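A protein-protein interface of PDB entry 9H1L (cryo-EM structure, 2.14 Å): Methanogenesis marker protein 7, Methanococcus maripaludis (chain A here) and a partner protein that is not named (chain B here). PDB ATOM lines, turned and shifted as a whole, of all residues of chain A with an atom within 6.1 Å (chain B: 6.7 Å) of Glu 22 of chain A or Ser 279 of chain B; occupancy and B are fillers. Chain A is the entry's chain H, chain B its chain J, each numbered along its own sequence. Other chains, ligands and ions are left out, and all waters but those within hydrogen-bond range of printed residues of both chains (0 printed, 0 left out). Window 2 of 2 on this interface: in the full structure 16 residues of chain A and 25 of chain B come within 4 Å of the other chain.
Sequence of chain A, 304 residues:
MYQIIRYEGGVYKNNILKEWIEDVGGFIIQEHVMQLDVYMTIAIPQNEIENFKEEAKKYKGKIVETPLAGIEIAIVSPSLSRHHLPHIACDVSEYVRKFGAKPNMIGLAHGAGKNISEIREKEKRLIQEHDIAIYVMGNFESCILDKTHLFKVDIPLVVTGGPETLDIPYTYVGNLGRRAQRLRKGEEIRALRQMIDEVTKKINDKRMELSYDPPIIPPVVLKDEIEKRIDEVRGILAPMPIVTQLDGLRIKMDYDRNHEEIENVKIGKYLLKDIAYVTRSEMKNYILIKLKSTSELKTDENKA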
ATOM      1  N   LEU A  17     -18.832   2.271  -2.324  1.00  0.00           N
ATOM      2  CA  LEU A  17     -19.902   1.279  -2.338  1.00  0.00           C
ATOM      3  C   LEU A  17     -21.145   1.779  -1.610  1.00  0.00           C
ATOM      4  O   LEU A  17     -22.269   1.494  -2.043  1.00  0.00           O
ATOM      5  CB  LEU A  17     -19.412  -0.030  -1.722  1.00  0.00           C
ATOM      6  CG  LEU A  17     -20.391  -1.203  -1.758  1.00  0.00           C
ATOM      7  CD1 LEU A  17     -20.355  -1.888  -3.112  1.00  0.00           C
ATOM      8  CD2 LEU A  17     -20.085  -2.187  -0.650  1.00  0.00           C
ATOM      9  N   LYS A  18     -20.966   2.519  -0.512  1.00  0.00           N
ATOM     10  CA  LYS A  18     -22.103   3.135   0.165  1.00  0.00           C
ATOM     11  C   LYS A  18     -22.794   4.157  -0.728  1.00  0.00           C
ATOM     12  O   LYS A  18     -24.025   4.264  -0.724  1.00  0.00           O
ATOM     13  CB  LYS A  18     -21.643   3.789   1.465  1.00  0.00           C
ATOM     14  CG  LYS A  18     -21.228   2.816   2.548  1.00  0.00           C
ATOM     15  CD  LYS A  18     -21.878   3.172   3.866  1.00  0.00           C
ATOM     16  CE  LYS A  18     -21.145   4.320   4.530  1.00  0.00           C
ATOM     17  NZ  LYS A  18     -19.879   3.871   5.166  1.00  0.00           N
ATOM     18  N   GLU A  19     -22.012   4.917  -1.499  1.00  0.00           N
ATOM     19  CA  GLU A  19     -22.586   5.856  -2.456  1.00  0.00           C
ATOM     20  C   GLU A  19     -23.358   5.132  -3.550  1.00  0.00           C
ATOM     21  O   GLU A  19     -24.416   5.597  -3.979  1.00  0.00           O
ATOM     22  CB  GLU A  19     -21.488   6.727  -3.064  1.00  0.00           C
ATOM     23  CG  GLU A  19     -20.939   7.775  -2.121  1.00  0.00           C
ATOM     24  CD  GLU A  19     -19.854   8.610  -2.760  1.00  0.00           C
ATOM     25  OE1 GLU A  19     -19.910   8.814  -3.990  1.00  0.00           O
ATOM     26  OE2 GLU A  19     -18.938   9.050  -2.037  1.00  0.00           O
ATOM     27  N   TRP A  20     -22.836   3.995  -4.020  1.00  0.00           N
ATOM     28  CA  TRP A  20     -23.556   3.192  -5.010  1.00  0.00           C
ATOM     29  C   TRP A  20     -24.867   2.662  -4.444  1.00  0.00           C
ATOM     30  O   TRP A  20     -25.893   2.651  -5.138  1.00  0.00           O
ATOM     31  CB  TRP A  20     -22.677   2.038  -5.489  1.00  0.00           C
ATOM     32  CG  TRP A  20     -23.234   1.290  -6.666  1.00  0.00           C
ATOM     33  CD1 TRP A  20     -22.971   1.527  -7.983  1.00  0.00           C
ATOM     34  CD2 TRP A  20     -24.138   0.178  -6.633  1.00  0.00           C
ATOM     35  NE1 TRP A  20     -23.655   0.637  -8.772  1.00  0.00           N
ATOM     36  CE2 TRP A  20     -24.379  -0.201  -7.968  1.00  0.00           C
ATOM     37  CE3 TRP A  20     -24.767  -0.533  -5.608  1.00  0.00           C
ATOM     38  CZ2 TRP A  20     -25.223  -1.258  -8.303  1.00  0.00           C
ATOM     39  CZ3 TRP A  20     -25.606  -1.580  -5.941  1.00  0.00           C
ATOM     40  CH2 TRP A  20     -25.825  -1.932  -7.276  1.00  0.00           C
ATOM     41  N   ILE A  21     -24.845   2.217  -3.187  1.00  0.00           N
ATOM     42  CA  ILE A  21     -26.053   1.738  -2.517  1.00  0.00           C
ATOM     43  C   ILE A  21     -27.077   2.860  -2.396  1.00  0.00           C
ATOM     44  O   ILE A  21     -28.272   2.661  -2.648  1.00  0.00           O
ATOM     45  CB  ILE A  21     -25.683   1.146  -1.142  1.00  0.00           C
ATOM     46  CG1 ILE A  21     -25.073  -0.246  -1.307  1.00  0.00           C
ATOM     47  CG2 ILE A  21     -26.884   1.100  -0.218  1.00  0.00           C
ATOM     48  CD1 ILE A  21     -24.282  -0.708  -0.106  1.00  0.00           C
ATOM     49  N   GLU A  22     -26.622   4.058  -2.026  1.00  0.00           N
ATOM     50  CA  GLU A  22     -27.521   5.204  -1.927  1.00  0.00           C
ATOM     51  C   GLU A  22     -28.062   5.609  -3.295  1.00  0.00           C
ATOM     52  O   GLU A  22     -29.218   6.035  -3.409  1.00  0.00           O
ATOM     53  CB  GLU A  22     -26.793   6.371  -1.259  1.00  0.00           C
ATOM     54  CG  GLU A  22     -27.630   7.620  -1.077  1.00  0.00           C
ATOM     55  CD  GLU A  22     -27.227   8.419   0.145  1.00  0.00           C
ATOM     56  OE1 GLU A  22     -26.025   8.422   0.484  1.00  0.00           O
ATOM     57  OE2 GLU A  22     -28.111   9.044   0.765  1.00  0.00           O
ATOM     58  N   ASP A  23     -27.245   5.477  -4.342  1.00  0.00           N
ATOM     59  CA  ASP A  23     -27.686   5.825  -5.691  1.00  0.00           C
ATOM     60  C   ASP A  23     -28.749   4.859  -6.199  1.00  0.00           C
ATOM     61  O   ASP A  23     -29.724   5.278  -6.832  1.00  0.00           O
ATOM     62  CB  ASP A  23     -26.494   5.855  -6.645  1.00  0.00           C
ATOM     63  CG  ASP A  23     -25.610   7.064  -6.429  1.00  0.00           C
ATOM     64  OD1 ASP A  23     -26.043   8.005  -5.735  1.00  0.00           O
ATOM     65  OD2 ASP A  23     -24.481   7.075  -6.958  1.00  0.00           O
ATOM     66  N   VAL A  24     -28.582   3.558  -5.933  1.00  0.00           N
ATOM     67  CA  VAL A  24     -29.572   2.580  -6.388  1.00  0.00           C
ATOM     68  C   VAL A  24     -30.772   2.483  -5.464  1.00  0.00           C
ATOM     69  O   VAL A  24     -31.654   1.647  -5.698  1.00  0.00           O
ATOM     70  CB  VAL A  24     -28.956   1.175  -6.554  1.00  0.00           C
ATOM     71  CG1 VAL A  24     -27.763   1.227  -7.487  1.00  0.00           C
ATOM     72  CG2 VAL A  24     -28.561   0.597  -5.207  1.00  0.00           C
ATOM     73  N   GLY A  25     -30.839   3.310  -4.426  1.00  0.00           N
ATOM     74  CA  GLY A  25     -31.976   3.324  -3.533  1.00  0.00           C
ATOM     75  C   GLY A  25     -31.883   2.404  -2.337  1.00  0.00           C
ATOM     76  O   GLY A  25     -32.873   2.262  -1.611  1.00  0.00           O
ATOM     77  N   GLY A  26     -30.734   1.776  -2.107  1.00  0.00           N
ATOM     78  CA  GLY A  26     -30.584   0.922  -0.948  1.00  0.00           C
ATOM     79  C   GLY A  26     -30.436   1.713   0.337  1.00  0.00           C
ATOM     80  O   GLY A  26     -30.137   2.906   0.344  1.00  0.00           O
ATOM     81  N   ILE A  28     -28.648   1.433   4.270  1.00  0.00           N
ATOM     82  CA  ILE A  28     -27.716   0.754   5.165  1.00  0.00           C
ATOM     83  C   ILE A  28     -28.385   0.675   6.535  1.00  0.00           C
ATOM     84  O   ILE A  28     -28.546   1.682   7.224  1.00  0.00           O
ATOM     85  CB  ILE A  28     -26.361   1.464   5.231  1.00  0.00           C
ATOM     86  CG1 ILE A  28     -25.661   1.397   3.872  1.00  0.00           C
ATOM     87  CG2 ILE A  28     -25.485   0.834   6.300  1.00  0.00           C
ATOM     88  CD1 ILE A  28     -25.687   2.695   3.103  1.00  0.00           C
ATOM     89  N   TYR B 231     -31.428   3.657 -12.502  1.00  0.00           N
ATOM     90  CA  TYR B 231     -31.040   4.984 -12.950  1.00  0.00           C
ATOM     91  C   TYR B 231     -30.020   4.888 -14.075  1.00  0.00           C
ATOM     92  O   TYR B 231     -29.464   3.826 -14.361  1.00  0.00           O
ATOM     93  CB  TYR B 231     -30.470   5.826 -11.797  1.00  0.00           C
ATOM     94  CG  TYR B 231     -29.126   5.354 -11.276  1.00  0.00           C
ATOM     95  CD1 TYR B 231     -27.943   5.744 -11.889  1.00  0.00           C
ATOM     96  CD2 TYR B 231     -29.042   4.528 -10.165  1.00  0.00           C
ATOM     97  CE1 TYR B 231     -26.719   5.318 -11.420  1.00  0.00           C
ATOM     98  CE2 TYR B 231     -27.822   4.098  -9.688  1.00  0.00           C
ATOM     99  CZ  TYR B 231     -26.664   4.496 -10.320  1.00  0.00           C
ATOM    100  OH  TYR B 231     -25.444   4.072  -9.849  1.00  0.00           O
ATOM    101  N   GLU B 245     -29.281  21.374  -1.126  1.00  0.00           N
ATOM    102  CA  GLU B 245     -30.023  20.179  -0.747  1.00  0.00           C
ATOM    103  C   GLU B 245     -31.471  20.316  -1.197  1.00  0.00           C
ATOM    104  O   GLU B 245     -32.149  21.284  -0.841  1.00  0.00           O
ATOM    105  CB  GLU B 245     -29.966  19.935   0.766  1.00  0.00           C
ATOM    106  CG  GLU B 245     -28.884  18.958   1.233  1.00  0.00           C
ATOM    107  CD  GLU B 245     -27.469  19.512   1.165  1.00  0.00           C
ATOM    108  OE1 GLU B 245     -27.253  20.572   0.546  1.00  0.00           O
ATOM    109  OE2 GLU B 245     -26.563  18.875   1.741  1.00  0.00           O
ATOM    110  N   PRO B 247     -33.949  17.385  -0.912  1.00  0.00           N
ATOM    111  CA  PRO B 247     -34.235  15.967  -0.612  1.00  0.00           C
ATOM    112  C   PRO B 247     -35.717  15.587  -0.635  1.00  0.00           C
ATOM    113  O   PRO B 247     -36.388  15.450   0.389  1.00  0.00           O
ATOM    114  CB  PRO B 247     -33.641  15.803   0.787  1.00  0.00           C
ATOM    115  CG  PRO B 247     -33.815  17.154   1.418  1.00  0.00           C
ATOM    116  CD  PRO B 247     -33.845  18.191   0.317  1.00  0.00           C
ATOM    117  N   ARG B 250     -37.305  10.545  -5.260  1.00  0.00           N
ATOM    118  CA  ARG B 250     -36.713  10.296  -6.572  1.00  0.00           C
ATOM    119  C   ARG B 250     -37.666   9.394  -7.353  1.00  0.00           C
ATOM    120  O   ARG B 250     -37.470   8.184  -7.485  1.00  0.00           O
ATOM    121  CB  ARG B 250     -35.330   9.674  -6.427  1.00  0.00           C
ATOM    122  CG  ARG B 250     -34.336  10.548  -5.686  1.00  0.00           C
ATOM    123  CD  ARG B 250     -33.024   9.820  -5.458  1.00  0.00           C
ATOM    124  NE  ARG B 250     -33.128   8.831  -4.392  1.00  0.00           N
ATOM    125  CZ  ARG B 250     -32.165   7.982  -4.064  1.00  0.00           C
ATOM    126  NH1 ARG B 250     -31.009   7.966  -4.704  1.00  0.00           N
ATOM    127  NH2 ARG B 250     -32.368   7.125  -3.067  1.00  0.00           N
ATOM    128  N   THR B 256     -31.693  14.196 -10.856  1.00  0.00           N
ATOM    129  CA  THR B 256     -31.007  14.583  -9.636  1.00  0.00           C
ATOM    130  C   THR B 256     -29.531  14.829  -9.917  1.00  0.00           C
ATOM    131  O   THR B 256     -28.957  14.286 -10.864  1.00  0.00           O
ATOM    132  CB  THR B 256     -31.136  13.511  -8.542  1.00  0.00           C
ATOM    133  OG1 THR B 256     -30.111  12.525  -8.715  1.00  0.00           O
ATOM    134  CG2 THR B 256     -32.491  12.832  -8.600  1.00  0.00           C
ATOM    135  N   VAL B 257     -28.924  15.662  -9.078  1.00  0.00           N
ATOM    136  CA  VAL B 257     -27.488  15.911  -9.098  1.00  0.00           C
ATOM    137  C   VAL B 257     -26.929  15.540  -7.733  1.00  0.00           C
ATOM    138  O   VAL B 257     -27.385  16.059  -6.709  1.00  0.00           O
ATOM    139  CB  VAL B 257     -27.164  17.377  -9.436  1.00  0.00           C
ATOM    140  CG1 VAL B 257     -25.666  17.562  -9.586  1.00  0.00           C
ATOM    141  CG2 VAL B 257     -27.880  17.796 -10.705  1.00  0.00           C
ATOM    142  N   ARG B 258     -25.948  14.643  -7.720  1.00  0.00           N
ATOM    143  CA  ARG B 258     -25.308  14.250  -6.472  1.00  0.00           C
ATOM    144  C   ARG B 258     -24.416  15.383  -5.985  1.00  0.00           C
ATOM    145  O   ARG B 258     -23.558  15.871  -6.723  1.00  0.00           O
ATOM    146  CB  ARG B 258     -24.494  12.973  -6.669  1.00  0.00           C
ATOM    147  CG  ARG B 258     -23.727  12.531  -5.440  1.00  0.00           C
ATOM    148  CD  ARG B 258     -23.163  11.135  -5.623  1.00  0.00           C
ATOM    149  NE  ARG B 258     -23.981  10.126  -4.966  1.00  0.00           N
ATOM    150  CZ  ARG B 258     -23.914   9.833  -3.675  1.00  0.00           C
ATOM    151  NH1 ARG B 258     -23.072  10.460  -2.869  1.00  0.00           N
ATOM    152  NH2 ARG B 258     -24.710   8.891  -3.181  1.00  0.00           N
ATOM    153  N   ASN B 259     -24.624  15.806  -4.739  1.00  0.00           N
ATOM    154  CA  ASN B 259     -23.987  17.006  -4.216  1.00  0.00           C
ATOM    155  C   ASN B 259     -22.868  16.723  -3.225  1.00  0.00           C
ATOM    156  O   ASN B 259     -22.277  17.672  -2.701  1.00  0.00           O
ATOM    157  CB  ASN B 259     -25.035  17.907  -3.559  1.00  0.00           C
ATOM    158  CG  ASN B 259     -25.839  17.189  -2.497  1.00  0.00           C
ATOM    159  OD1 ASN B 259     -25.603  16.017  -2.210  1.00  0.00           O
ATOM    160  ND2 ASN B 259     -26.796  17.890  -1.907  1.00  0.00           N
ATOM    161  N   ILE B 260     -22.557  15.459  -2.950  1.00  0.00           N
ATOM    162  CA  ILE B 260     -21.545  15.120  -1.959  1.00  0.00           C
ATOM    163  C   ILE B 260     -20.985  13.744  -2.283  1.00  0.00           C
ATOM    164  O   ILE B 260     -21.673  12.891  -2.849  1.00  0.00           O
ATOM    165  CB  ILE B 260     -22.118  15.171  -0.522  1.00  0.00           C
ATOM    166  CG1 ILE B 260     -20.986  15.234   0.506  1.00  0.00           C
ATOM    167  CG2 ILE B 260     -23.021  13.979  -0.252  1.00  0.00           C
ATOM    168  CD1 ILE B 260     -20.082  16.438   0.341  1.00  0.00           C
ATOM    169  N   GLY B 261     -19.718  13.544  -1.953  1.00  0.00           N
ATOM    170  CA  GLY B 261     -19.083  12.253  -2.067  1.00  0.00           C
ATOM    171  C   GLY B 261     -18.122  12.170  -3.235  1.00  0.00           C
ATOM    172  O   GLY B 261     -17.688  13.175  -3.802  1.00  0.00           O
ATOM    173  N   TYR B 268     -28.230  12.268 -12.470  1.00  0.00           N
ATOM    174  CA  TYR B 268     -28.950  11.003 -12.495  1.00  0.00           C
ATOM    175  C   TYR B 268     -30.337  11.200 -13.085  1.00  0.00           C
ATOM    176  O   TYR B 268     -30.969  12.239 -12.872  1.00  0.00           O
ATOM    177  CB  TYR B 268     -29.084  10.414 -11.087  1.00  0.00           C
ATOM    178  CG  TYR B 268     -27.781  10.060 -10.415  1.00  0.00           C
ATOM    179  CD1 TYR B 268     -27.003  11.033  -9.806  1.00  0.00           C
ATOM    180  CD2 TYR B 268     -27.340   8.748 -10.368  1.00  0.00           C
ATOM    181  CE1 TYR B 268     -25.818  10.709  -9.184  1.00  0.00           C
ATOM    182  CE2 TYR B 268     -26.157   8.416  -9.749  1.00  0.00           C
ATOM    183  CZ  TYR B 268     -25.400   9.399  -9.158  1.00  0.00           C
ATOM    184  OH  TYR B 268     -24.218   9.070  -8.538  1.00  0.00           O
ATOM    185  N   TYR B 270     -33.766   8.793 -12.983  1.00  0.00           N
ATOM    186  CA  TYR B 270     -34.234   7.594 -12.300  1.00  0.00           C
ATOM    187  C   TYR B 270     -35.354   6.927 -13.086  1.00  0.00           C
ATOM    188  O   TYR B 270     -36.334   7.578 -13.459  1.00  0.00           O
ATOM    189  CB  TYR B 270     -34.711   7.935 -10.888  1.00  0.00           C
ATOM    190  CG  TYR B 270     -33.604   7.919  -9.861  1.00  0.00           C
ATOM    191  CD1 TYR B 270     -32.747   9.001  -9.718  1.00  0.00           C
ATOM    192  CD2 TYR B 270     -33.408   6.817  -9.042  1.00  0.00           C
ATOM    193  CE1 TYR B 270     -31.733   8.988  -8.784  1.00  0.00           C
ATOM    194  CE2 TYR B 270     -32.395   6.796  -8.107  1.00  0.00           C
ATOM    195  CZ  TYR B 270     -31.561   7.884  -7.983  1.00  0.00           C
ATOM    196  OH  TYR B 270     -30.552   7.865  -7.050  1.00  0.00           O
ATOM    197  N   ALA B 275     -36.847   6.211  -2.778  1.00  0.00           N
ATOM    198  CA  ALA B 275     -37.016   7.110  -1.649  1.00  0.00           C
ATOM    199  C   ALA B 275     -36.123   8.340  -1.795  1.00  0.00           C
ATOM    200  O   ALA B 275     -35.199   8.384  -2.609  1.00  0.00           O
ATOM    201  CB  ALA B 275     -36.712   6.385  -0.340  1.00  0.00           C
ATOM    202  N   SER B 276     -36.417   9.351  -0.984  1.00  0.00           N
ATOM    203  CA  SER B 276     -35.617  10.565  -0.970  1.00  0.00           C
ATOM    204  C   SER B 276     -34.218  10.285  -0.432  1.00  0.00           C
ATOM    205  O   SER B 276     -34.007   9.375   0.372  1.00  0.00           O
ATOM    206  CB  SER B 276     -36.296  11.639  -0.121  1.00  0.00           C
ATOM    207  OG  SER B 276     -35.392  12.676   0.204  1.00  0.00           O
ATOM    208  N   SER B 277     -33.255  11.078  -0.893  1.00  0.00           N
ATOM    209  CA  SER B 277     -31.871  10.954  -0.463  1.00  0.00           C
ATOM    210  C   SER B 277     -31.303  12.330  -0.157  1.00  0.00           C
ATOM    211  O   SER B 277     -31.557  13.293  -0.886  1.00  0.00           O
ATOM    212  CB  SER B 277     -31.016  10.263  -1.530  1.00  0.00           C
ATOM    213  OG  SER B 277     -29.659  10.200  -1.131  1.00  0.00           O
ATOM    214  N   LEU B 278     -30.534  12.419   0.929  1.00  0.00           N
ATOM    215  CA  LEU B 278     -29.893  13.678   1.285  1.00  0.00           C
ATOM    216  C   LEU B 278     -28.714  14.002   0.379  1.00  0.00           C
ATOM    217  O   LEU B 278     -28.303  15.164   0.312  1.00  0.00           O
ATOM    218  CB  LEU B 278     -29.431  13.643   2.743  1.00  0.00           C
ATOM    219  CG  LEU B 278     -30.287  14.406   3.754  1.00  0.00           C
ATOM    220  CD1 LEU B 278     -30.061  15.901   3.626  1.00  0.00           C
ATOM    221  CD2 LEU B 278     -31.760  14.064   3.592  1.00  0.00           C
ATOM    222  N   SER B 279     -28.163  13.009  -0.313  1.00  0.00           N
ATOM    223  CA  SER B 279     -27.018  13.207  -1.190  1.00  0.00           C
ATOM    224  C   SER B 279     -27.416  13.486  -2.631  1.00  0.00           C
ATOM    225  O   SER B 279     -26.534  13.621  -3.484  1.00  0.00           O
ATOM    226  CB  SER B 279     -26.101  11.983  -1.144  1.00  0.00           C
ATOM    227  OG  SER B 279     -25.975  11.492   0.178  1.00  0.00           O
ATOM    228  N   HIS B 280     -28.710  13.573  -2.926  1.00  0.00           N
ATOM    229  CA  HIS B 280     -29.193  13.824  -4.275  1.00  0.00           C
ATOM    230  C   HIS B 280     -30.041  15.086  -4.278  1.00  0.00           C
ATOM    231  O   HIS B 280     -31.001  15.196  -3.509  1.00  0.00           O
ATOM    232  CB  HIS B 280     -30.003  12.636  -4.798  1.00  0.00           C
ATOM    233  CG  HIS B 280     -29.162  11.472  -5.214  1.00  0.00           C
ATOM    234  ND1 HIS B 280     -28.828  11.227  -6.528  1.00  0.00           N
ATOM    235  CD2 HIS B 280     -28.582  10.487  -4.490  1.00  0.00           C
ATOM    236  CE1 HIS B 280     -28.080  10.141  -6.595  1.00  0.00           C
ATOM    237  NE2 HIS B 280     -27.916   9.673  -5.371  1.00  0.00           N
ATOM    238  N   THR B 281     -29.685  16.029  -5.144  1.00  0.00           N
ATOM    239  CA  THR B 281     -30.410  17.284  -5.302  1.00  0.00           C
ATOM    240  C   THR B 281     -31.232  17.194  -6.580  1.00  0.00           C
ATOM    241  O   THR B 281     -30.675  17.215  -7.682  1.00  0.00           O
ATOM    242  CB  THR B 281     -29.450  18.469  -5.350  1.00  0.00           C
ATOM    243  OG1 THR B 281     -28.564  18.419  -4.225  1.00  0.00           O
ATOM    244  CG2 THR B 281     -30.217  19.779  -5.325  1.00  0.00           C
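The side-chain carboxylate of Asp 23 of chain A lies within salt-bridge range of the guanidinium group of Arg 258 of chain B, at 3.0 Å.
The side-chain carboxylate (OD2) of Asp 23 of chain A lies within hydrogen-bond range of the side-chain hydroxyl (OH) of Tyr 268 of chain B (2.6 Å).
The side-chain hydroxyl (OG) of Ser 277 of chain B sits at hydrogen-bond distance from the side-chain carboxylate (OE2) of Glu 22 of chain A, at 2.7 Å.
OG of Ser 279 of chain B lies within hydrogen-bond range of OE1 of Glu 22 of chain A, at 3.1 Å.
OE1 of Glu 19 of chain A is in salt-bridge range of NH1 of Arg 258 of chain B (3.7 Å).
A ring nitrogen (NE2) of His 280 of chain B sits at hydrogen-bond distance from the side-chain carboxylate of Asp 23 of chain A, 2.5 Å away.
The side-chain hydroxyl (OH) of Tyr 270 of chain B lies within hydrogen-bond range of the backbone carbonyl oxygen (O) of Asp 23 of chain A (2.7 Å).
The guanidinium group of Arg 250 of chain B is in hydrogen-bond range of the backbone carbonyl oxygen of Glu 22 of chain A, at 2.9 Å.
The guanidinium group of Arg 258 of chain B is in salt-bridge range of the side-chain carboxylate of Glu 22 of chain A (3.9 Å).
O of Thr 256 of chain B is in hydrogen-bond range of N of Tyr 268 of chain B (2.7 Å).
OD1 of Asn 259 of chain B lies close to O of Ser 279 of chain B (2.9 Å).
The side-chain hydroxyl (OG) of Ser 277 of chain B sits close to the backbone NH (N) of Ser 279 of chain B, at 3.3 Å.
OG1 of Thr 256 of chain B sits at hydrogen-bond distance from ND1 of His 280 of chain B, at 2.8 Å.
The guanidinium group (NE) of Arg 250 of chain B sits at hydrogen-bond distance from the backbone carbonyl oxygen (O) of Ala 275 of chain B, at 2.8 Å.
The backbone carbonyl oxygen (O) of Ile 260 of chain B lies within hydrogen-bond range of the guanidinium group (NH1) of Arg 258 of chain B (2.8 Å).
Gly 261 of chain B touches Glu 19 of chain A (CA to OE2, 3.2 Å).
CD2 of Tyr 231 of chain B touches O of Asp 23 of chain A (3.5 Å).
Arg 250 of chain B touches Asp 23 of chain A (NH1 to O, 3.7 Å).
Tyr 231 of chain B touches Val 24 of chain A.
CA of Gly 25 of chain A touches NH2 of Arg 250 of chain B, 3.8 Å away.
Of the printed residues of chain B, Glu 19 of chain A touches Arg 258 and Gly 261.
Of chain B, only Arg 250 (2.9 Å), Arg 258 (3.8 Å), Ser 277 (2.7 Å) and Ser 279 (3.1 Å) come within 4 Å of Glu 22 of chain A.
Printed residues of chain B within 4 Å of Gly 25 of chain A: Arg 250 (3.8 Å).
Of the printed residues of chain A, Tyr 231 of chain B touches Asp 23 and Val 24.
Asn 259 of chain B touches none of the printed residues of chain A.
Of the printed residues of chain A, Gly 261 of chain B touches Glu 19.
Of chain A, only Glu 22 comes within 4 Å of Ser 279 of chain B.
The nearest residue of chain B that does not touch Glu 22 of chain A is Leu 278 of chain B (4.2 Å).
The nearest printed residue of chain A that does not touch Ser 279 of chain B is Asp 23 of chain A (6.1 Å).
Of the 11 printed residues of chain A, 5 touch a printed residue of chain B.
Among the printed residues, Asp or Glu carboxylates within 4 Å of a Lys or Arg side-chain nitrogen of the other chain: Glu 19 of chain A with Arg 258 of chain B, Glu 22 of chain A with Arg 258 of chain B and Asp 23 of chain A with Arg 258 of chain B.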
